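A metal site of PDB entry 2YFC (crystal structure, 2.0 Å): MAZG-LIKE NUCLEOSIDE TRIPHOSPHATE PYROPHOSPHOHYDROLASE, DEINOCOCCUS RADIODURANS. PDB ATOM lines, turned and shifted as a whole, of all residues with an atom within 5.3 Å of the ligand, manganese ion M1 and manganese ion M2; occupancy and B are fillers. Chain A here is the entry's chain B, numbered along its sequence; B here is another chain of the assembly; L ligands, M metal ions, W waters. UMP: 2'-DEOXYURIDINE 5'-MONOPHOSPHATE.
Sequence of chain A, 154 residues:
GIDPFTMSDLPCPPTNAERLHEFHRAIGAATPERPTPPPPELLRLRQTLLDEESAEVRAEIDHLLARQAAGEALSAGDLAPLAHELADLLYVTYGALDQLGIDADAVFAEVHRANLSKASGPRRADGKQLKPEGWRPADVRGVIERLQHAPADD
The side-chain amino group (NZ) of Lys 128 of chain B is in salt-bridge range of an oxygen (OP3) of the ligand (3.4 Å). The side-chain amino group (NZ) of Lys 118 of chain B sits at hydrogen-bond distance from an oxygen (O4') of the ligand. The side-chain amide nitrogen (ND2) of Asn 115 of chain B is in hydrogen-bond range of an oxygen (O3') of the ligand (3.1 Å). The side-chain carboxylate (OD1) of Asp 88 sits at hydrogen-bond distance from an oxygen (O3') of the ligand (2.5 Å). OP2 of the ligand is in salt-bridge range of NZ of Lys 131 of chain B (2.9 Å). The backbone NH of Gln 129 of chain B is in hydrogen-bond range of an oxygen (O4) of the ligand, 2.8 Å away.
OE1 of Glu 52 lies within salt-bridge range of NZ of Lys 128 of chain B. The backbone carbonyl oxygen (O) of Val 92 is in hydrogen-bond range of the guanidinium group (NH2) of Arg 46. OD1 of Asn 115 of chain B lies within hydrogen-bond range of NZ of Lys 118 of chain B (2.9 Å). The side-chain amide nitrogen (NE2) of Gln 129 of chain B sits at hydrogen-bond distance from the backbone carbonyl oxygen (O) of Lys 118 of chain B (3.1 Å).
Residues that only touch the ligand: Tyr 91, Val 92, Phe 23, Val 111 of chain B and Gly 127 of chain B. Hydrophobic or aromatic side chains that line the ligand: Phe 23, Tyr 91, Val 92 and Val 111 of chain B. Within 4 Å of the ligand: Phe 23, Glu 52, Glu 53, Asp 88, Tyr 91, Val 92, Val 111 of chain B, Asn 115 of chain B, Lys 118 of chain B, Gly 127 of chain B, Lys 128 of chain B, Gln 129 of chain B and Lys 131 of chain B.
Within 4 Å of manganese ion M1: Glu 52, Glu 53 and Glu 56.
Four residues have an atom within 4 Å of manganese ion M2: Glu 53, Glu 56, Glu 85 and Asp 88.
Manganese ion M1 is bound by water W6 (2.2 Å), the side-chain carboxylate (OE2) of Glu 52 (2.2 Å), an oxygen (OP1) of the ligand (2.2 Å), the side-chain carboxylate (OE2) of Glu 53 (2.3 Å), the side-chain carboxylate (OE2) of Glu 56 (2.3 Å) and water W7 (2.4 Å). Manganese ion M1 has six donor atoms within binding distance.
Manganese ion M2 is bound by OE1 of Glu 53 (2.1 Å), water W6 (2.1 Å), OE1 of Glu 56 (2.2 Å), OE1 of Glu 85 (2.2 Å) and OD2 of Asp 88 (2.2 Å).
Water W3 lies within hydrogen-bond range of O2 of the ligand, NH2 of Arg 46 and NE2 of His 24. Water W2 bridges an oxygen (OP2) of the ligand (2.7 Å) and the side-chain amino group (NZ) of Lys 118 of chain B (2.7 Å). Water W5 lies within hydrogen-bond range of OP3 of the ligand, O of Gln 129 of chain B and NZ of Lys 118 of chain B. Water W8 lies within hydrogen-bond range of N3 of the ligand (2.8 Å), NE2 of His 24 (2.8 Å) and NH1 of Arg 46 (2.9 Å). Water W1 lies within hydrogen-bond range of an oxygen (O4) of the ligand (2.9 Å) and the backbone carbonyl oxygen of Gly 127 of chain B (3.3 Å).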
ATOM      1  N   LEU A  20      -3.226  34.470  -4.667  1.00  0.00           N
ATOM      2  CA  LEU A  20      -3.783  33.330  -3.935  1.00  0.00           C
ATOM      3  C   LEU A  20      -5.146  33.696  -3.359  1.00  0.00           C
ATOM      4  O   LEU A  20      -6.084  32.898  -3.367  1.00  0.00           O
ATOM      5  CB  LEU A  20      -2.849  32.842  -2.821  1.00  0.00           C
ATOM      6  CG  LEU A  20      -2.108  31.526  -3.127  1.00  0.00           C
ATOM      7  CD1 LEU A  20      -3.114  30.401  -3.424  1.00  0.00           C
ATOM      8  CD2 LEU A  20      -1.185  31.736  -4.306  1.00  0.00           C
ATOM      9  N   PHE A  23      -7.563  33.406  -6.051  1.00  0.00           N
ATOM     10  CA  PHE A  23      -7.859  31.986  -6.295  1.00  0.00           C
ATOM     11  C   PHE A  23      -8.820  31.376  -5.271  1.00  0.00           C
ATOM     12  O   PHE A  23      -9.810  30.728  -5.642  1.00  0.00           O
ATOM     13  CB  PHE A  23      -6.538  31.191  -6.338  1.00  0.00           C
ATOM     14  CG  PHE A  23      -6.726  29.692  -6.430  1.00  0.00           C
ATOM     15  CD1 PHE A  23      -7.208  29.105  -7.604  1.00  0.00           C
ATOM     16  CD2 PHE A  23      -6.400  28.875  -5.366  1.00  0.00           C
ATOM     17  CE1 PHE A  23      -7.370  27.725  -7.698  1.00  0.00           C
ATOM     18  CE2 PHE A  23      -6.552  27.498  -5.450  1.00  0.00           C
ATOM     19  CZ  PHE A  23      -7.042  26.914  -6.619  1.00  0.00           C
ATOM     20  N   HIS A  24      -8.549  31.582  -3.994  1.00  0.00           N
ATOM     21  CA  HIS A  24      -9.408  31.002  -2.955  1.00  0.00           C
ATOM     22  C   HIS A  24     -10.834  31.561  -2.958  1.00  0.00           C
ATOM     23  O   HIS A  24     -11.798  30.822  -2.726  1.00  0.00           O
ATOM     24  CB  HIS A  24      -8.739  31.105  -1.585  1.00  0.00           C
ATOM     25  CG  HIS A  24      -7.600  30.136  -1.430  1.00  0.00           C
ATOM     26  ND1 HIS A  24      -6.574  30.320  -0.527  1.00  0.00           N
ATOM     27  CD2 HIS A  24      -7.324  28.990  -2.092  1.00  0.00           C
ATOM     28  CE1 HIS A  24      -5.721  29.306  -0.627  1.00  0.00           C
ATOM     29  NE2 HIS A  24      -6.152  28.491  -1.571  1.00  0.00           N
ATOM     30  N   ILE A  27     -12.685  29.769  -5.810  1.00  0.00           N
ATOM     31  CA  ILE A  27     -13.043  28.378  -5.613  1.00  0.00           C
ATOM     32  C   ILE A  27     -13.831  28.160  -4.330  1.00  0.00           C
ATOM     33  O   ILE A  27     -14.162  27.032  -3.984  1.00  0.00           O
ATOM     34  CB  ILE A  27     -11.809  27.438  -5.651  1.00  0.00           C
ATOM     35  CG1 ILE A  27     -10.925  27.675  -4.420  1.00  0.00           C
ATOM     36  CG2 ILE A  27     -10.999  27.664  -6.928  1.00  0.00           C
ATOM     37  CD1 ILE A  27      -9.893  26.576  -4.225  1.00  0.00           C
ATOM     38  N   LEU A  45      -4.974  19.339   4.938  1.00  0.00           N
ATOM     39  CA  LEU A  45      -4.926  19.631   3.510  1.00  0.00           C
ATOM     40  C   LEU A  45      -3.651  20.381   3.148  1.00  0.00           C
ATOM     41  O   LEU A  45      -3.008  20.043   2.159  1.00  0.00           O
ATOM     42  CB  LEU A  45      -6.151  20.419   3.028  1.00  0.00           C
ATOM     43  CG  LEU A  45      -6.072  20.909   1.569  1.00  0.00           C
ATOM     44  CD1 LEU A  45      -6.154  19.728   0.607  1.00  0.00           C
ATOM     45  CD2 LEU A  45      -7.156  21.945   1.255  1.00  0.00           C
ATOM     46  N   ARG A  46      -3.268  21.401   3.926  1.00  0.00           N
ATOM     47  CA  ARG A  46      -2.080  22.166   3.531  1.00  0.00           C
ATOM     48  C   ARG A  46      -0.843  21.259   3.500  1.00  0.00           C
ATOM     49  O   ARG A  46       0.009  21.378   2.620  1.00  0.00           O
ATOM     50  CB  ARG A  46      -1.821  23.408   4.422  1.00  0.00           C
ATOM     51  CG  ARG A  46      -2.966  24.439   4.498  1.00  0.00           C
ATOM     52  CD  ARG A  46      -3.697  24.621   3.156  1.00  0.00           C
ATOM     53  NE  ARG A  46      -2.815  24.935   2.031  1.00  0.00           N
ATOM     54  CZ  ARG A  46      -3.256  25.385   0.852  1.00  0.00           C
ATOM     55  NH1 ARG A  46      -4.562  25.600   0.669  1.00  0.00           N
ATOM     56  NH2 ARG A  46      -2.402  25.627  -0.146  1.00  0.00           N
ATOM     57  N   LEU A  49      -0.837  19.033   0.319  1.00  0.00           N
ATOM     58  CA  LEU A  49      -0.486  19.747  -0.916  1.00  0.00           C
ATOM     59  C   LEU A  49       1.009  20.109  -0.916  1.00  0.00           C
ATOM     60  O   LEU A  49       1.655  20.040  -1.953  1.00  0.00           O
ATOM     61  CB  LEU A  49      -1.354  21.000  -1.072  1.00  0.00           C
ATOM     62  CG  LEU A  49      -2.868  20.774  -1.155  1.00  0.00           C
ATOM     63  CD1 LEU A  49      -3.597  22.121  -1.262  1.00  0.00           C
ATOM     64  CD2 LEU A  49      -3.242  19.846  -2.342  1.00  0.00           C
ATOM     65  N   GLU A  52       2.795  16.867  -1.726  1.00  0.00           N
ATOM     66  CA  GLU A  52       2.577  16.535  -3.131  1.00  0.00           C
ATOM     67  C   GLU A  52       3.455  17.356  -4.085  1.00  0.00           C
ATOM     68  O   GLU A  52       4.150  16.798  -4.947  1.00  0.00           O
ATOM     69  CB  GLU A  52       1.102  16.688  -3.513  1.00  0.00           C
ATOM     70  CG  GLU A  52       0.886  16.350  -4.978  1.00  0.00           C
ATOM     71  CD  GLU A  52      -0.497  16.742  -5.517  1.00  0.00           C
ATOM     72  OE1 GLU A  52      -1.449  17.022  -4.738  1.00  0.00           O
ATOM     73  OE2 GLU A  52      -0.607  16.751  -6.753  1.00  0.00           O
ATOM     74  N   GLU A  53       3.387  18.676  -3.970  1.00  0.00           N
ATOM     75  CA  GLU A  53       4.110  19.537  -4.903  1.00  0.00           C
ATOM     76  C   GLU A  53       5.626  19.490  -4.699  1.00  0.00           C
ATOM     77  O   GLU A  53       6.390  19.616  -5.658  1.00  0.00           O
ATOM     78  CB  GLU A  53       3.602  20.985  -4.879  1.00  0.00           C
ATOM     79  CG  GLU A  53       2.122  21.117  -5.259  1.00  0.00           C
ATOM     80  CD  GLU A  53       1.788  20.421  -6.565  1.00  0.00           C
ATOM     81  OE1 GLU A  53       2.466  20.661  -7.598  1.00  0.00           O
ATOM     82  OE2 GLU A  53       0.866  19.597  -6.559  1.00  0.00           O
ATOM     83  N   GLU A  56       6.897  16.485  -6.456  1.00  0.00           N
ATOM     84  CA  GLU A  56       6.994  16.773  -7.887  1.00  0.00           C
ATOM     85  C   GLU A  56       8.240  17.580  -8.260  1.00  0.00           C
ATOM     86  O   GLU A  56       8.838  17.354  -9.322  1.00  0.00           O
ATOM     87  CB  GLU A  56       5.728  17.495  -8.391  1.00  0.00           C
ATOM     88  CG  GLU A  56       4.506  16.606  -8.299  1.00  0.00           C
ATOM     89  CD  GLU A  56       3.216  17.324  -8.632  1.00  0.00           C
ATOM     90  OE1 GLU A  56       3.215  18.206  -9.502  1.00  0.00           O
ATOM     91  OE2 GLU A  56       2.196  16.972  -8.027  1.00  0.00           O
ATOM     92  N   GLU A  85       6.919  23.128 -11.645  1.00  0.00           N
ATOM     93  CA  GLU A  85       6.719  22.517 -10.333  1.00  0.00           C
ATOM     94  C   GLU A  85       7.182  23.430  -9.193  1.00  0.00           C
ATOM     95  O   GLU A  85       6.600  23.398  -8.114  1.00  0.00           O
ATOM     96  CB  GLU A  85       7.384  21.133 -10.256  1.00  0.00           C
ATOM     97  CG  GLU A  85       6.919  20.159 -11.355  1.00  0.00           C
ATOM     98  CD  GLU A  85       5.411  19.922 -11.343  1.00  0.00           C
ATOM     99  OE1 GLU A  85       4.724  20.478 -10.487  1.00  0.00           O
ATOM    100  OE2 GLU A  85       4.926  19.159 -12.195  1.00  0.00           O
ATOM    101  N   ALA A  87       6.942  26.688  -9.245  1.00  0.00           N
ATOM    102  CA  ALA A  87       5.852  27.648  -9.169  1.00  0.00           C
ATOM    103  C   ALA A  87       4.617  27.053  -8.460  1.00  0.00           C
ATOM    104  O   ALA A  87       3.969  27.744  -7.681  1.00  0.00           O
ATOM    105  CB  ALA A  87       5.481  28.137 -10.560  1.00  0.00           C
ATOM    106  N   ASP A  88       4.329  25.783  -8.727  1.00  0.00           N
ATOM    107  CA  ASP A  88       3.283  25.057  -7.973  1.00  0.00           C
ATOM    108  C   ASP A  88       3.584  24.976  -6.467  1.00  0.00           C
ATOM    109  O   ASP A  88       2.672  25.041  -5.628  1.00  0.00           O
ATOM    110  CB  ASP A  88       3.123  23.617  -8.520  1.00  0.00           C
ATOM    111  CG  ASP A  88       2.199  23.543  -9.726  1.00  0.00           C
ATOM    112  OD1 ASP A  88       1.650  24.594 -10.159  1.00  0.00           O
ATOM    113  OD2 ASP A  88       1.992  22.426 -10.241  1.00  0.00           O
ATOM    114  N   TYR A  91       2.942  28.194  -5.014  1.00  0.00           N
ATOM    115  CA  TYR A  91       1.497  28.430  -4.998  1.00  0.00           C
ATOM    116  C   TYR A  91       0.821  27.805  -3.760  1.00  0.00           C
ATOM    117  O   TYR A  91      -0.028  28.434  -3.123  1.00  0.00           O
ATOM    118  CB  TYR A  91       0.889  27.939  -6.304  1.00  0.00           C
ATOM    119  CG  TYR A  91      -0.383  28.665  -6.734  1.00  0.00           C
ATOM    120  CD1 TYR A  91      -1.633  28.298  -6.210  1.00  0.00           C
ATOM    121  CD2 TYR A  91      -0.354  29.680  -7.691  1.00  0.00           C
ATOM    122  CE1 TYR A  91      -2.793  28.956  -6.603  1.00  0.00           C
ATOM    123  CE2 TYR A  91      -1.519  30.343  -8.092  1.00  0.00           C
ATOM    124  CZ  TYR A  91      -2.734  29.969  -7.538  1.00  0.00           C
ATOM    125  OH  TYR A  91      -3.883  30.605  -7.925  1.00  0.00           O
ATOM    126  N   VAL A  92       1.193  26.585  -3.407  1.00  0.00           N
ATOM    127  CA  VAL A  92       0.603  25.950  -2.224  1.00  0.00           C
ATOM    128  C   VAL A  92       1.213  26.460  -0.906  1.00  0.00           C
ATOM    129  O   VAL A  92       0.610  26.300   0.152  1.00  0.00           O
ATOM    130  CB  VAL A  92       0.661  24.394  -2.266  1.00  0.00           C
ATOM    131  CG1 VAL A  92      -0.088  23.879  -3.456  1.00  0.00           C
ATOM    132  CG2 VAL A  92       2.129  23.876  -2.246  1.00  0.00           C
ATOM    133  N   VAL B 111       0.944  30.062 -14.264  1.00  0.00           N
ATOM    134  CA  VAL B 111       0.373  29.049 -13.373  1.00  0.00           C
ATOM    135  C   VAL B 111      -0.925  29.548 -12.690  1.00  0.00           C
ATOM    136  O   VAL B 111      -1.907  28.805 -12.597  1.00  0.00           O
ATOM    137  CB  VAL B 111       1.437  28.603 -12.330  1.00  0.00           C
ATOM    138  CG1 VAL B 111       0.794  27.816 -11.179  1.00  0.00           C
ATOM    139  CG2 VAL B 111       2.521  27.788 -13.025  1.00  0.00           C
ATOM    140  N   ASN B 115      -4.838  28.124 -12.839  1.00  0.00           N
ATOM    141  CA  ASN B 115      -5.465  27.757 -11.587  1.00  0.00           C
ATOM    142  C   ASN B 115      -6.859  28.369 -11.440  1.00  0.00           C
ATOM    143  O   ASN B 115      -7.725  27.764 -10.946  1.00  0.00           O
ATOM    144  CB  ASN B 115      -4.569  28.054 -10.415  1.00  0.00           C
ATOM    145  CG  ASN B 115      -3.507  26.961 -10.220  1.00  0.00           C
ATOM    146  OD1 ASN B 115      -3.608  25.961 -10.770  1.00  0.00           O
ATOM    147  ND2 ASN B 115      -2.544  27.220  -9.430  1.00  0.00           N
ATOM    148  N   LYS B 118      -9.712  26.519 -12.980  1.00  0.00           N
ATOM    149  CA  LYS B 118     -10.175  25.282 -12.353  1.00  0.00           C
ATOM    150  C   LYS B 118     -11.481  25.463 -11.575  1.00  0.00           C
ATOM    151  O   LYS B 118     -12.060  24.490 -11.091  1.00  0.00           O
ATOM    152  CB  LYS B 118      -9.121  24.713 -11.401  1.00  0.00           C
ATOM    153  CG  LYS B 118      -7.830  24.260 -12.062  1.00  0.00           C
ATOM    154  CD  LYS B 118      -6.751  23.919 -10.997  1.00  0.00           C
ATOM    155  CE  LYS B 118      -5.438  23.458 -11.676  1.00  0.00           C
ATOM    156  NZ  LYS B 118      -4.348  23.108 -10.677  1.00  0.00           N
ATOM    157  N   GLY B 127     -10.563  18.464   0.300  1.00  0.00           N
ATOM    158  CA  GLY B 127     -10.749  19.869  -0.033  1.00  0.00           C
ATOM    159  C   GLY B 127      -9.929  20.362  -1.215  1.00  0.00           C
ATOM    160  O   GLY B 127     -10.047  21.518  -1.621  1.00  0.00           O
ATOM    161  N   LYS B 128      -9.103  19.491  -1.776  1.00  0.00           N
ATOM    162  CA  LYS B 128      -8.300  19.899  -2.926  1.00  0.00           C
ATOM    163  C   LYS B 128      -9.189  20.180  -4.126  1.00  0.00           C
ATOM    164  O   LYS B 128     -10.081  19.401  -4.467  1.00  0.00           O
ATOM    165  CB  LYS B 128      -7.242  18.856  -3.321  1.00  0.00           C
ATOM    166  CG  LYS B 128      -6.383  19.299  -4.532  1.00  0.00           C
ATOM    167  CD  LYS B 128      -5.394  18.218  -4.980  1.00  0.00           C
ATOM    168  CE  LYS B 128      -4.459  18.734  -6.079  1.00  0.00           C
ATOM    169  NZ  LYS B 128      -3.467  17.702  -6.495  1.00  0.00           N
ATOM    170  N   GLN B 129      -8.933  21.317  -4.769  1.00  0.00           N
ATOM    171  CA  GLN B 129      -9.645  21.668  -5.994  1.00  0.00           C
ATOM    172  C   GLN B 129      -9.103  20.855  -7.167  1.00  0.00           C
ATOM    173  O   GLN B 129      -7.886  20.815  -7.389  1.00  0.00           O
ATOM    174  CB  GLN B 129      -9.457  23.171  -6.286  1.00  0.00           C
ATOM    175  CG  GLN B 129     -10.086  23.608  -7.594  1.00  0.00           C
ATOM    176  CD  GLN B 129     -11.579  23.446  -7.579  1.00  0.00           C
ATOM    177  OE1 GLN B 129     -12.196  23.966  -6.521  1.00  0.00           O
ATOM    178  NE2 GLN B 129     -12.169  22.830  -8.460  1.00  0.00           N
ATOM    179  N   LYS B 131      -9.511  19.482 -11.470  1.00  0.00           N
ATOM    180  CA  LYS B 131      -9.611  20.100 -12.795  1.00  0.00           C
ATOM    181  C   LYS B 131     -10.938  19.722 -13.472  1.00  0.00           C
ATOM    182  O   LYS B 131     -11.307  18.560 -13.474  1.00  0.00           O
ATOM    183  CB  LYS B 131      -8.423  19.623 -13.640  1.00  0.00           C
ATOM    184  CG  LYS B 131      -7.084  20.116 -13.079  1.00  0.00           C
ATOM    185  CD  LYS B 131      -5.898  19.215 -13.477  1.00  0.00           C
ATOM    186  CE  LYS B 131      -4.618  19.710 -12.775  1.00  0.00           C
ATOM    187  NZ  LYS B 131      -3.493  18.727 -12.847  1.00  0.00           N
HETATM  188  N1  UMP L   1      -3.902  24.187  -6.181  1.00  0.00           N
HETATM  189  C2  UMP L   1      -4.151  24.857  -5.043  1.00  0.00           C
HETATM  190  N3  UMP L   1      -5.193  24.427  -4.199  1.00  0.00           N
HETATM  191  C4  UMP L   1      -5.949  23.323  -4.543  1.00  0.00           C
HETATM  192  C5  UMP L   1      -5.695  22.602  -5.718  1.00  0.00           C
HETATM  193  C6  UMP L   1      -4.677  23.026  -6.539  1.00  0.00           C
HETATM  194  O2  UMP L   1      -3.479  25.827  -4.729  1.00  0.00           O
HETATM  195  O4  UMP L   1      -6.953  22.940  -3.688  1.00  0.00           O
HETATM  196  C1' UMP L   1      -2.809  24.602  -7.038  1.00  0.00           C
HETATM  197  C2' UMP L   1      -1.302  24.538  -6.654  1.00  0.00           C
HETATM  198  C3' UMP L   1      -0.612  24.242  -7.935  1.00  0.00           C
HETATM  199  C4' UMP L   1      -1.614  23.280  -8.549  1.00  0.00           C
HETATM  200  O3' UMP L   1      -0.228  25.351  -8.655  1.00  0.00           O
HETATM  201  O4' UMP L   1      -2.859  24.013  -8.418  1.00  0.00           O
HETATM  202  C5' UMP L   1      -1.659  21.831  -8.169  1.00  0.00           C
HETATM  203  O5' UMP L   1      -2.614  21.369  -9.060  1.00  0.00           O
HETATM  204  P   UMP L   1      -2.504  19.846  -9.416  1.00  0.00           P
HETATM  205  OP1 UMP L   1      -1.792  19.044  -8.374  1.00  0.00           O
HETATM  206  OP2 UMP L   1      -1.747  19.755 -10.703  1.00  0.00           O
HETATM  207  OP3 UMP L   1      -3.878  19.239  -9.488  1.00  0.00           O
HETATM  208 MN    MN M   1       0.244  18.151  -8.195  1.00  0.00          MN
HETATM  209 MN    MN M   2       2.634  20.349  -9.674  1.00  0.00          MN
HETATM  210  O   HOH W   1      -8.368  24.329  -1.634  1.00  0.00           O
HETATM  211  O   HOH W   2      -2.169  22.086 -11.970  1.00  0.00           O
HETATM  212  O   HOH W   3      -3.271  26.991  -2.425  1.00  0.00           O
HETATM  213  O   HOH W   4      -5.062  17.021 -10.128  1.00  0.00           O
HETATM  214  O   HOH W   5      -5.944  21.014  -9.363  1.00  0.00           O
HETATM  215  O   HOH W   6       0.807  19.308  -9.956  1.00  0.00           O
HETATM  216  O   HOH W   7      -0.489  16.479  -9.786  1.00  0.00           O
HETATM  217  O   HOH W   8      -6.036  25.665  -1.863  1.00  0.00           O
HETATM  218  O   HOH W   9       1.843  20.972 -12.775  1.00  0.00           O
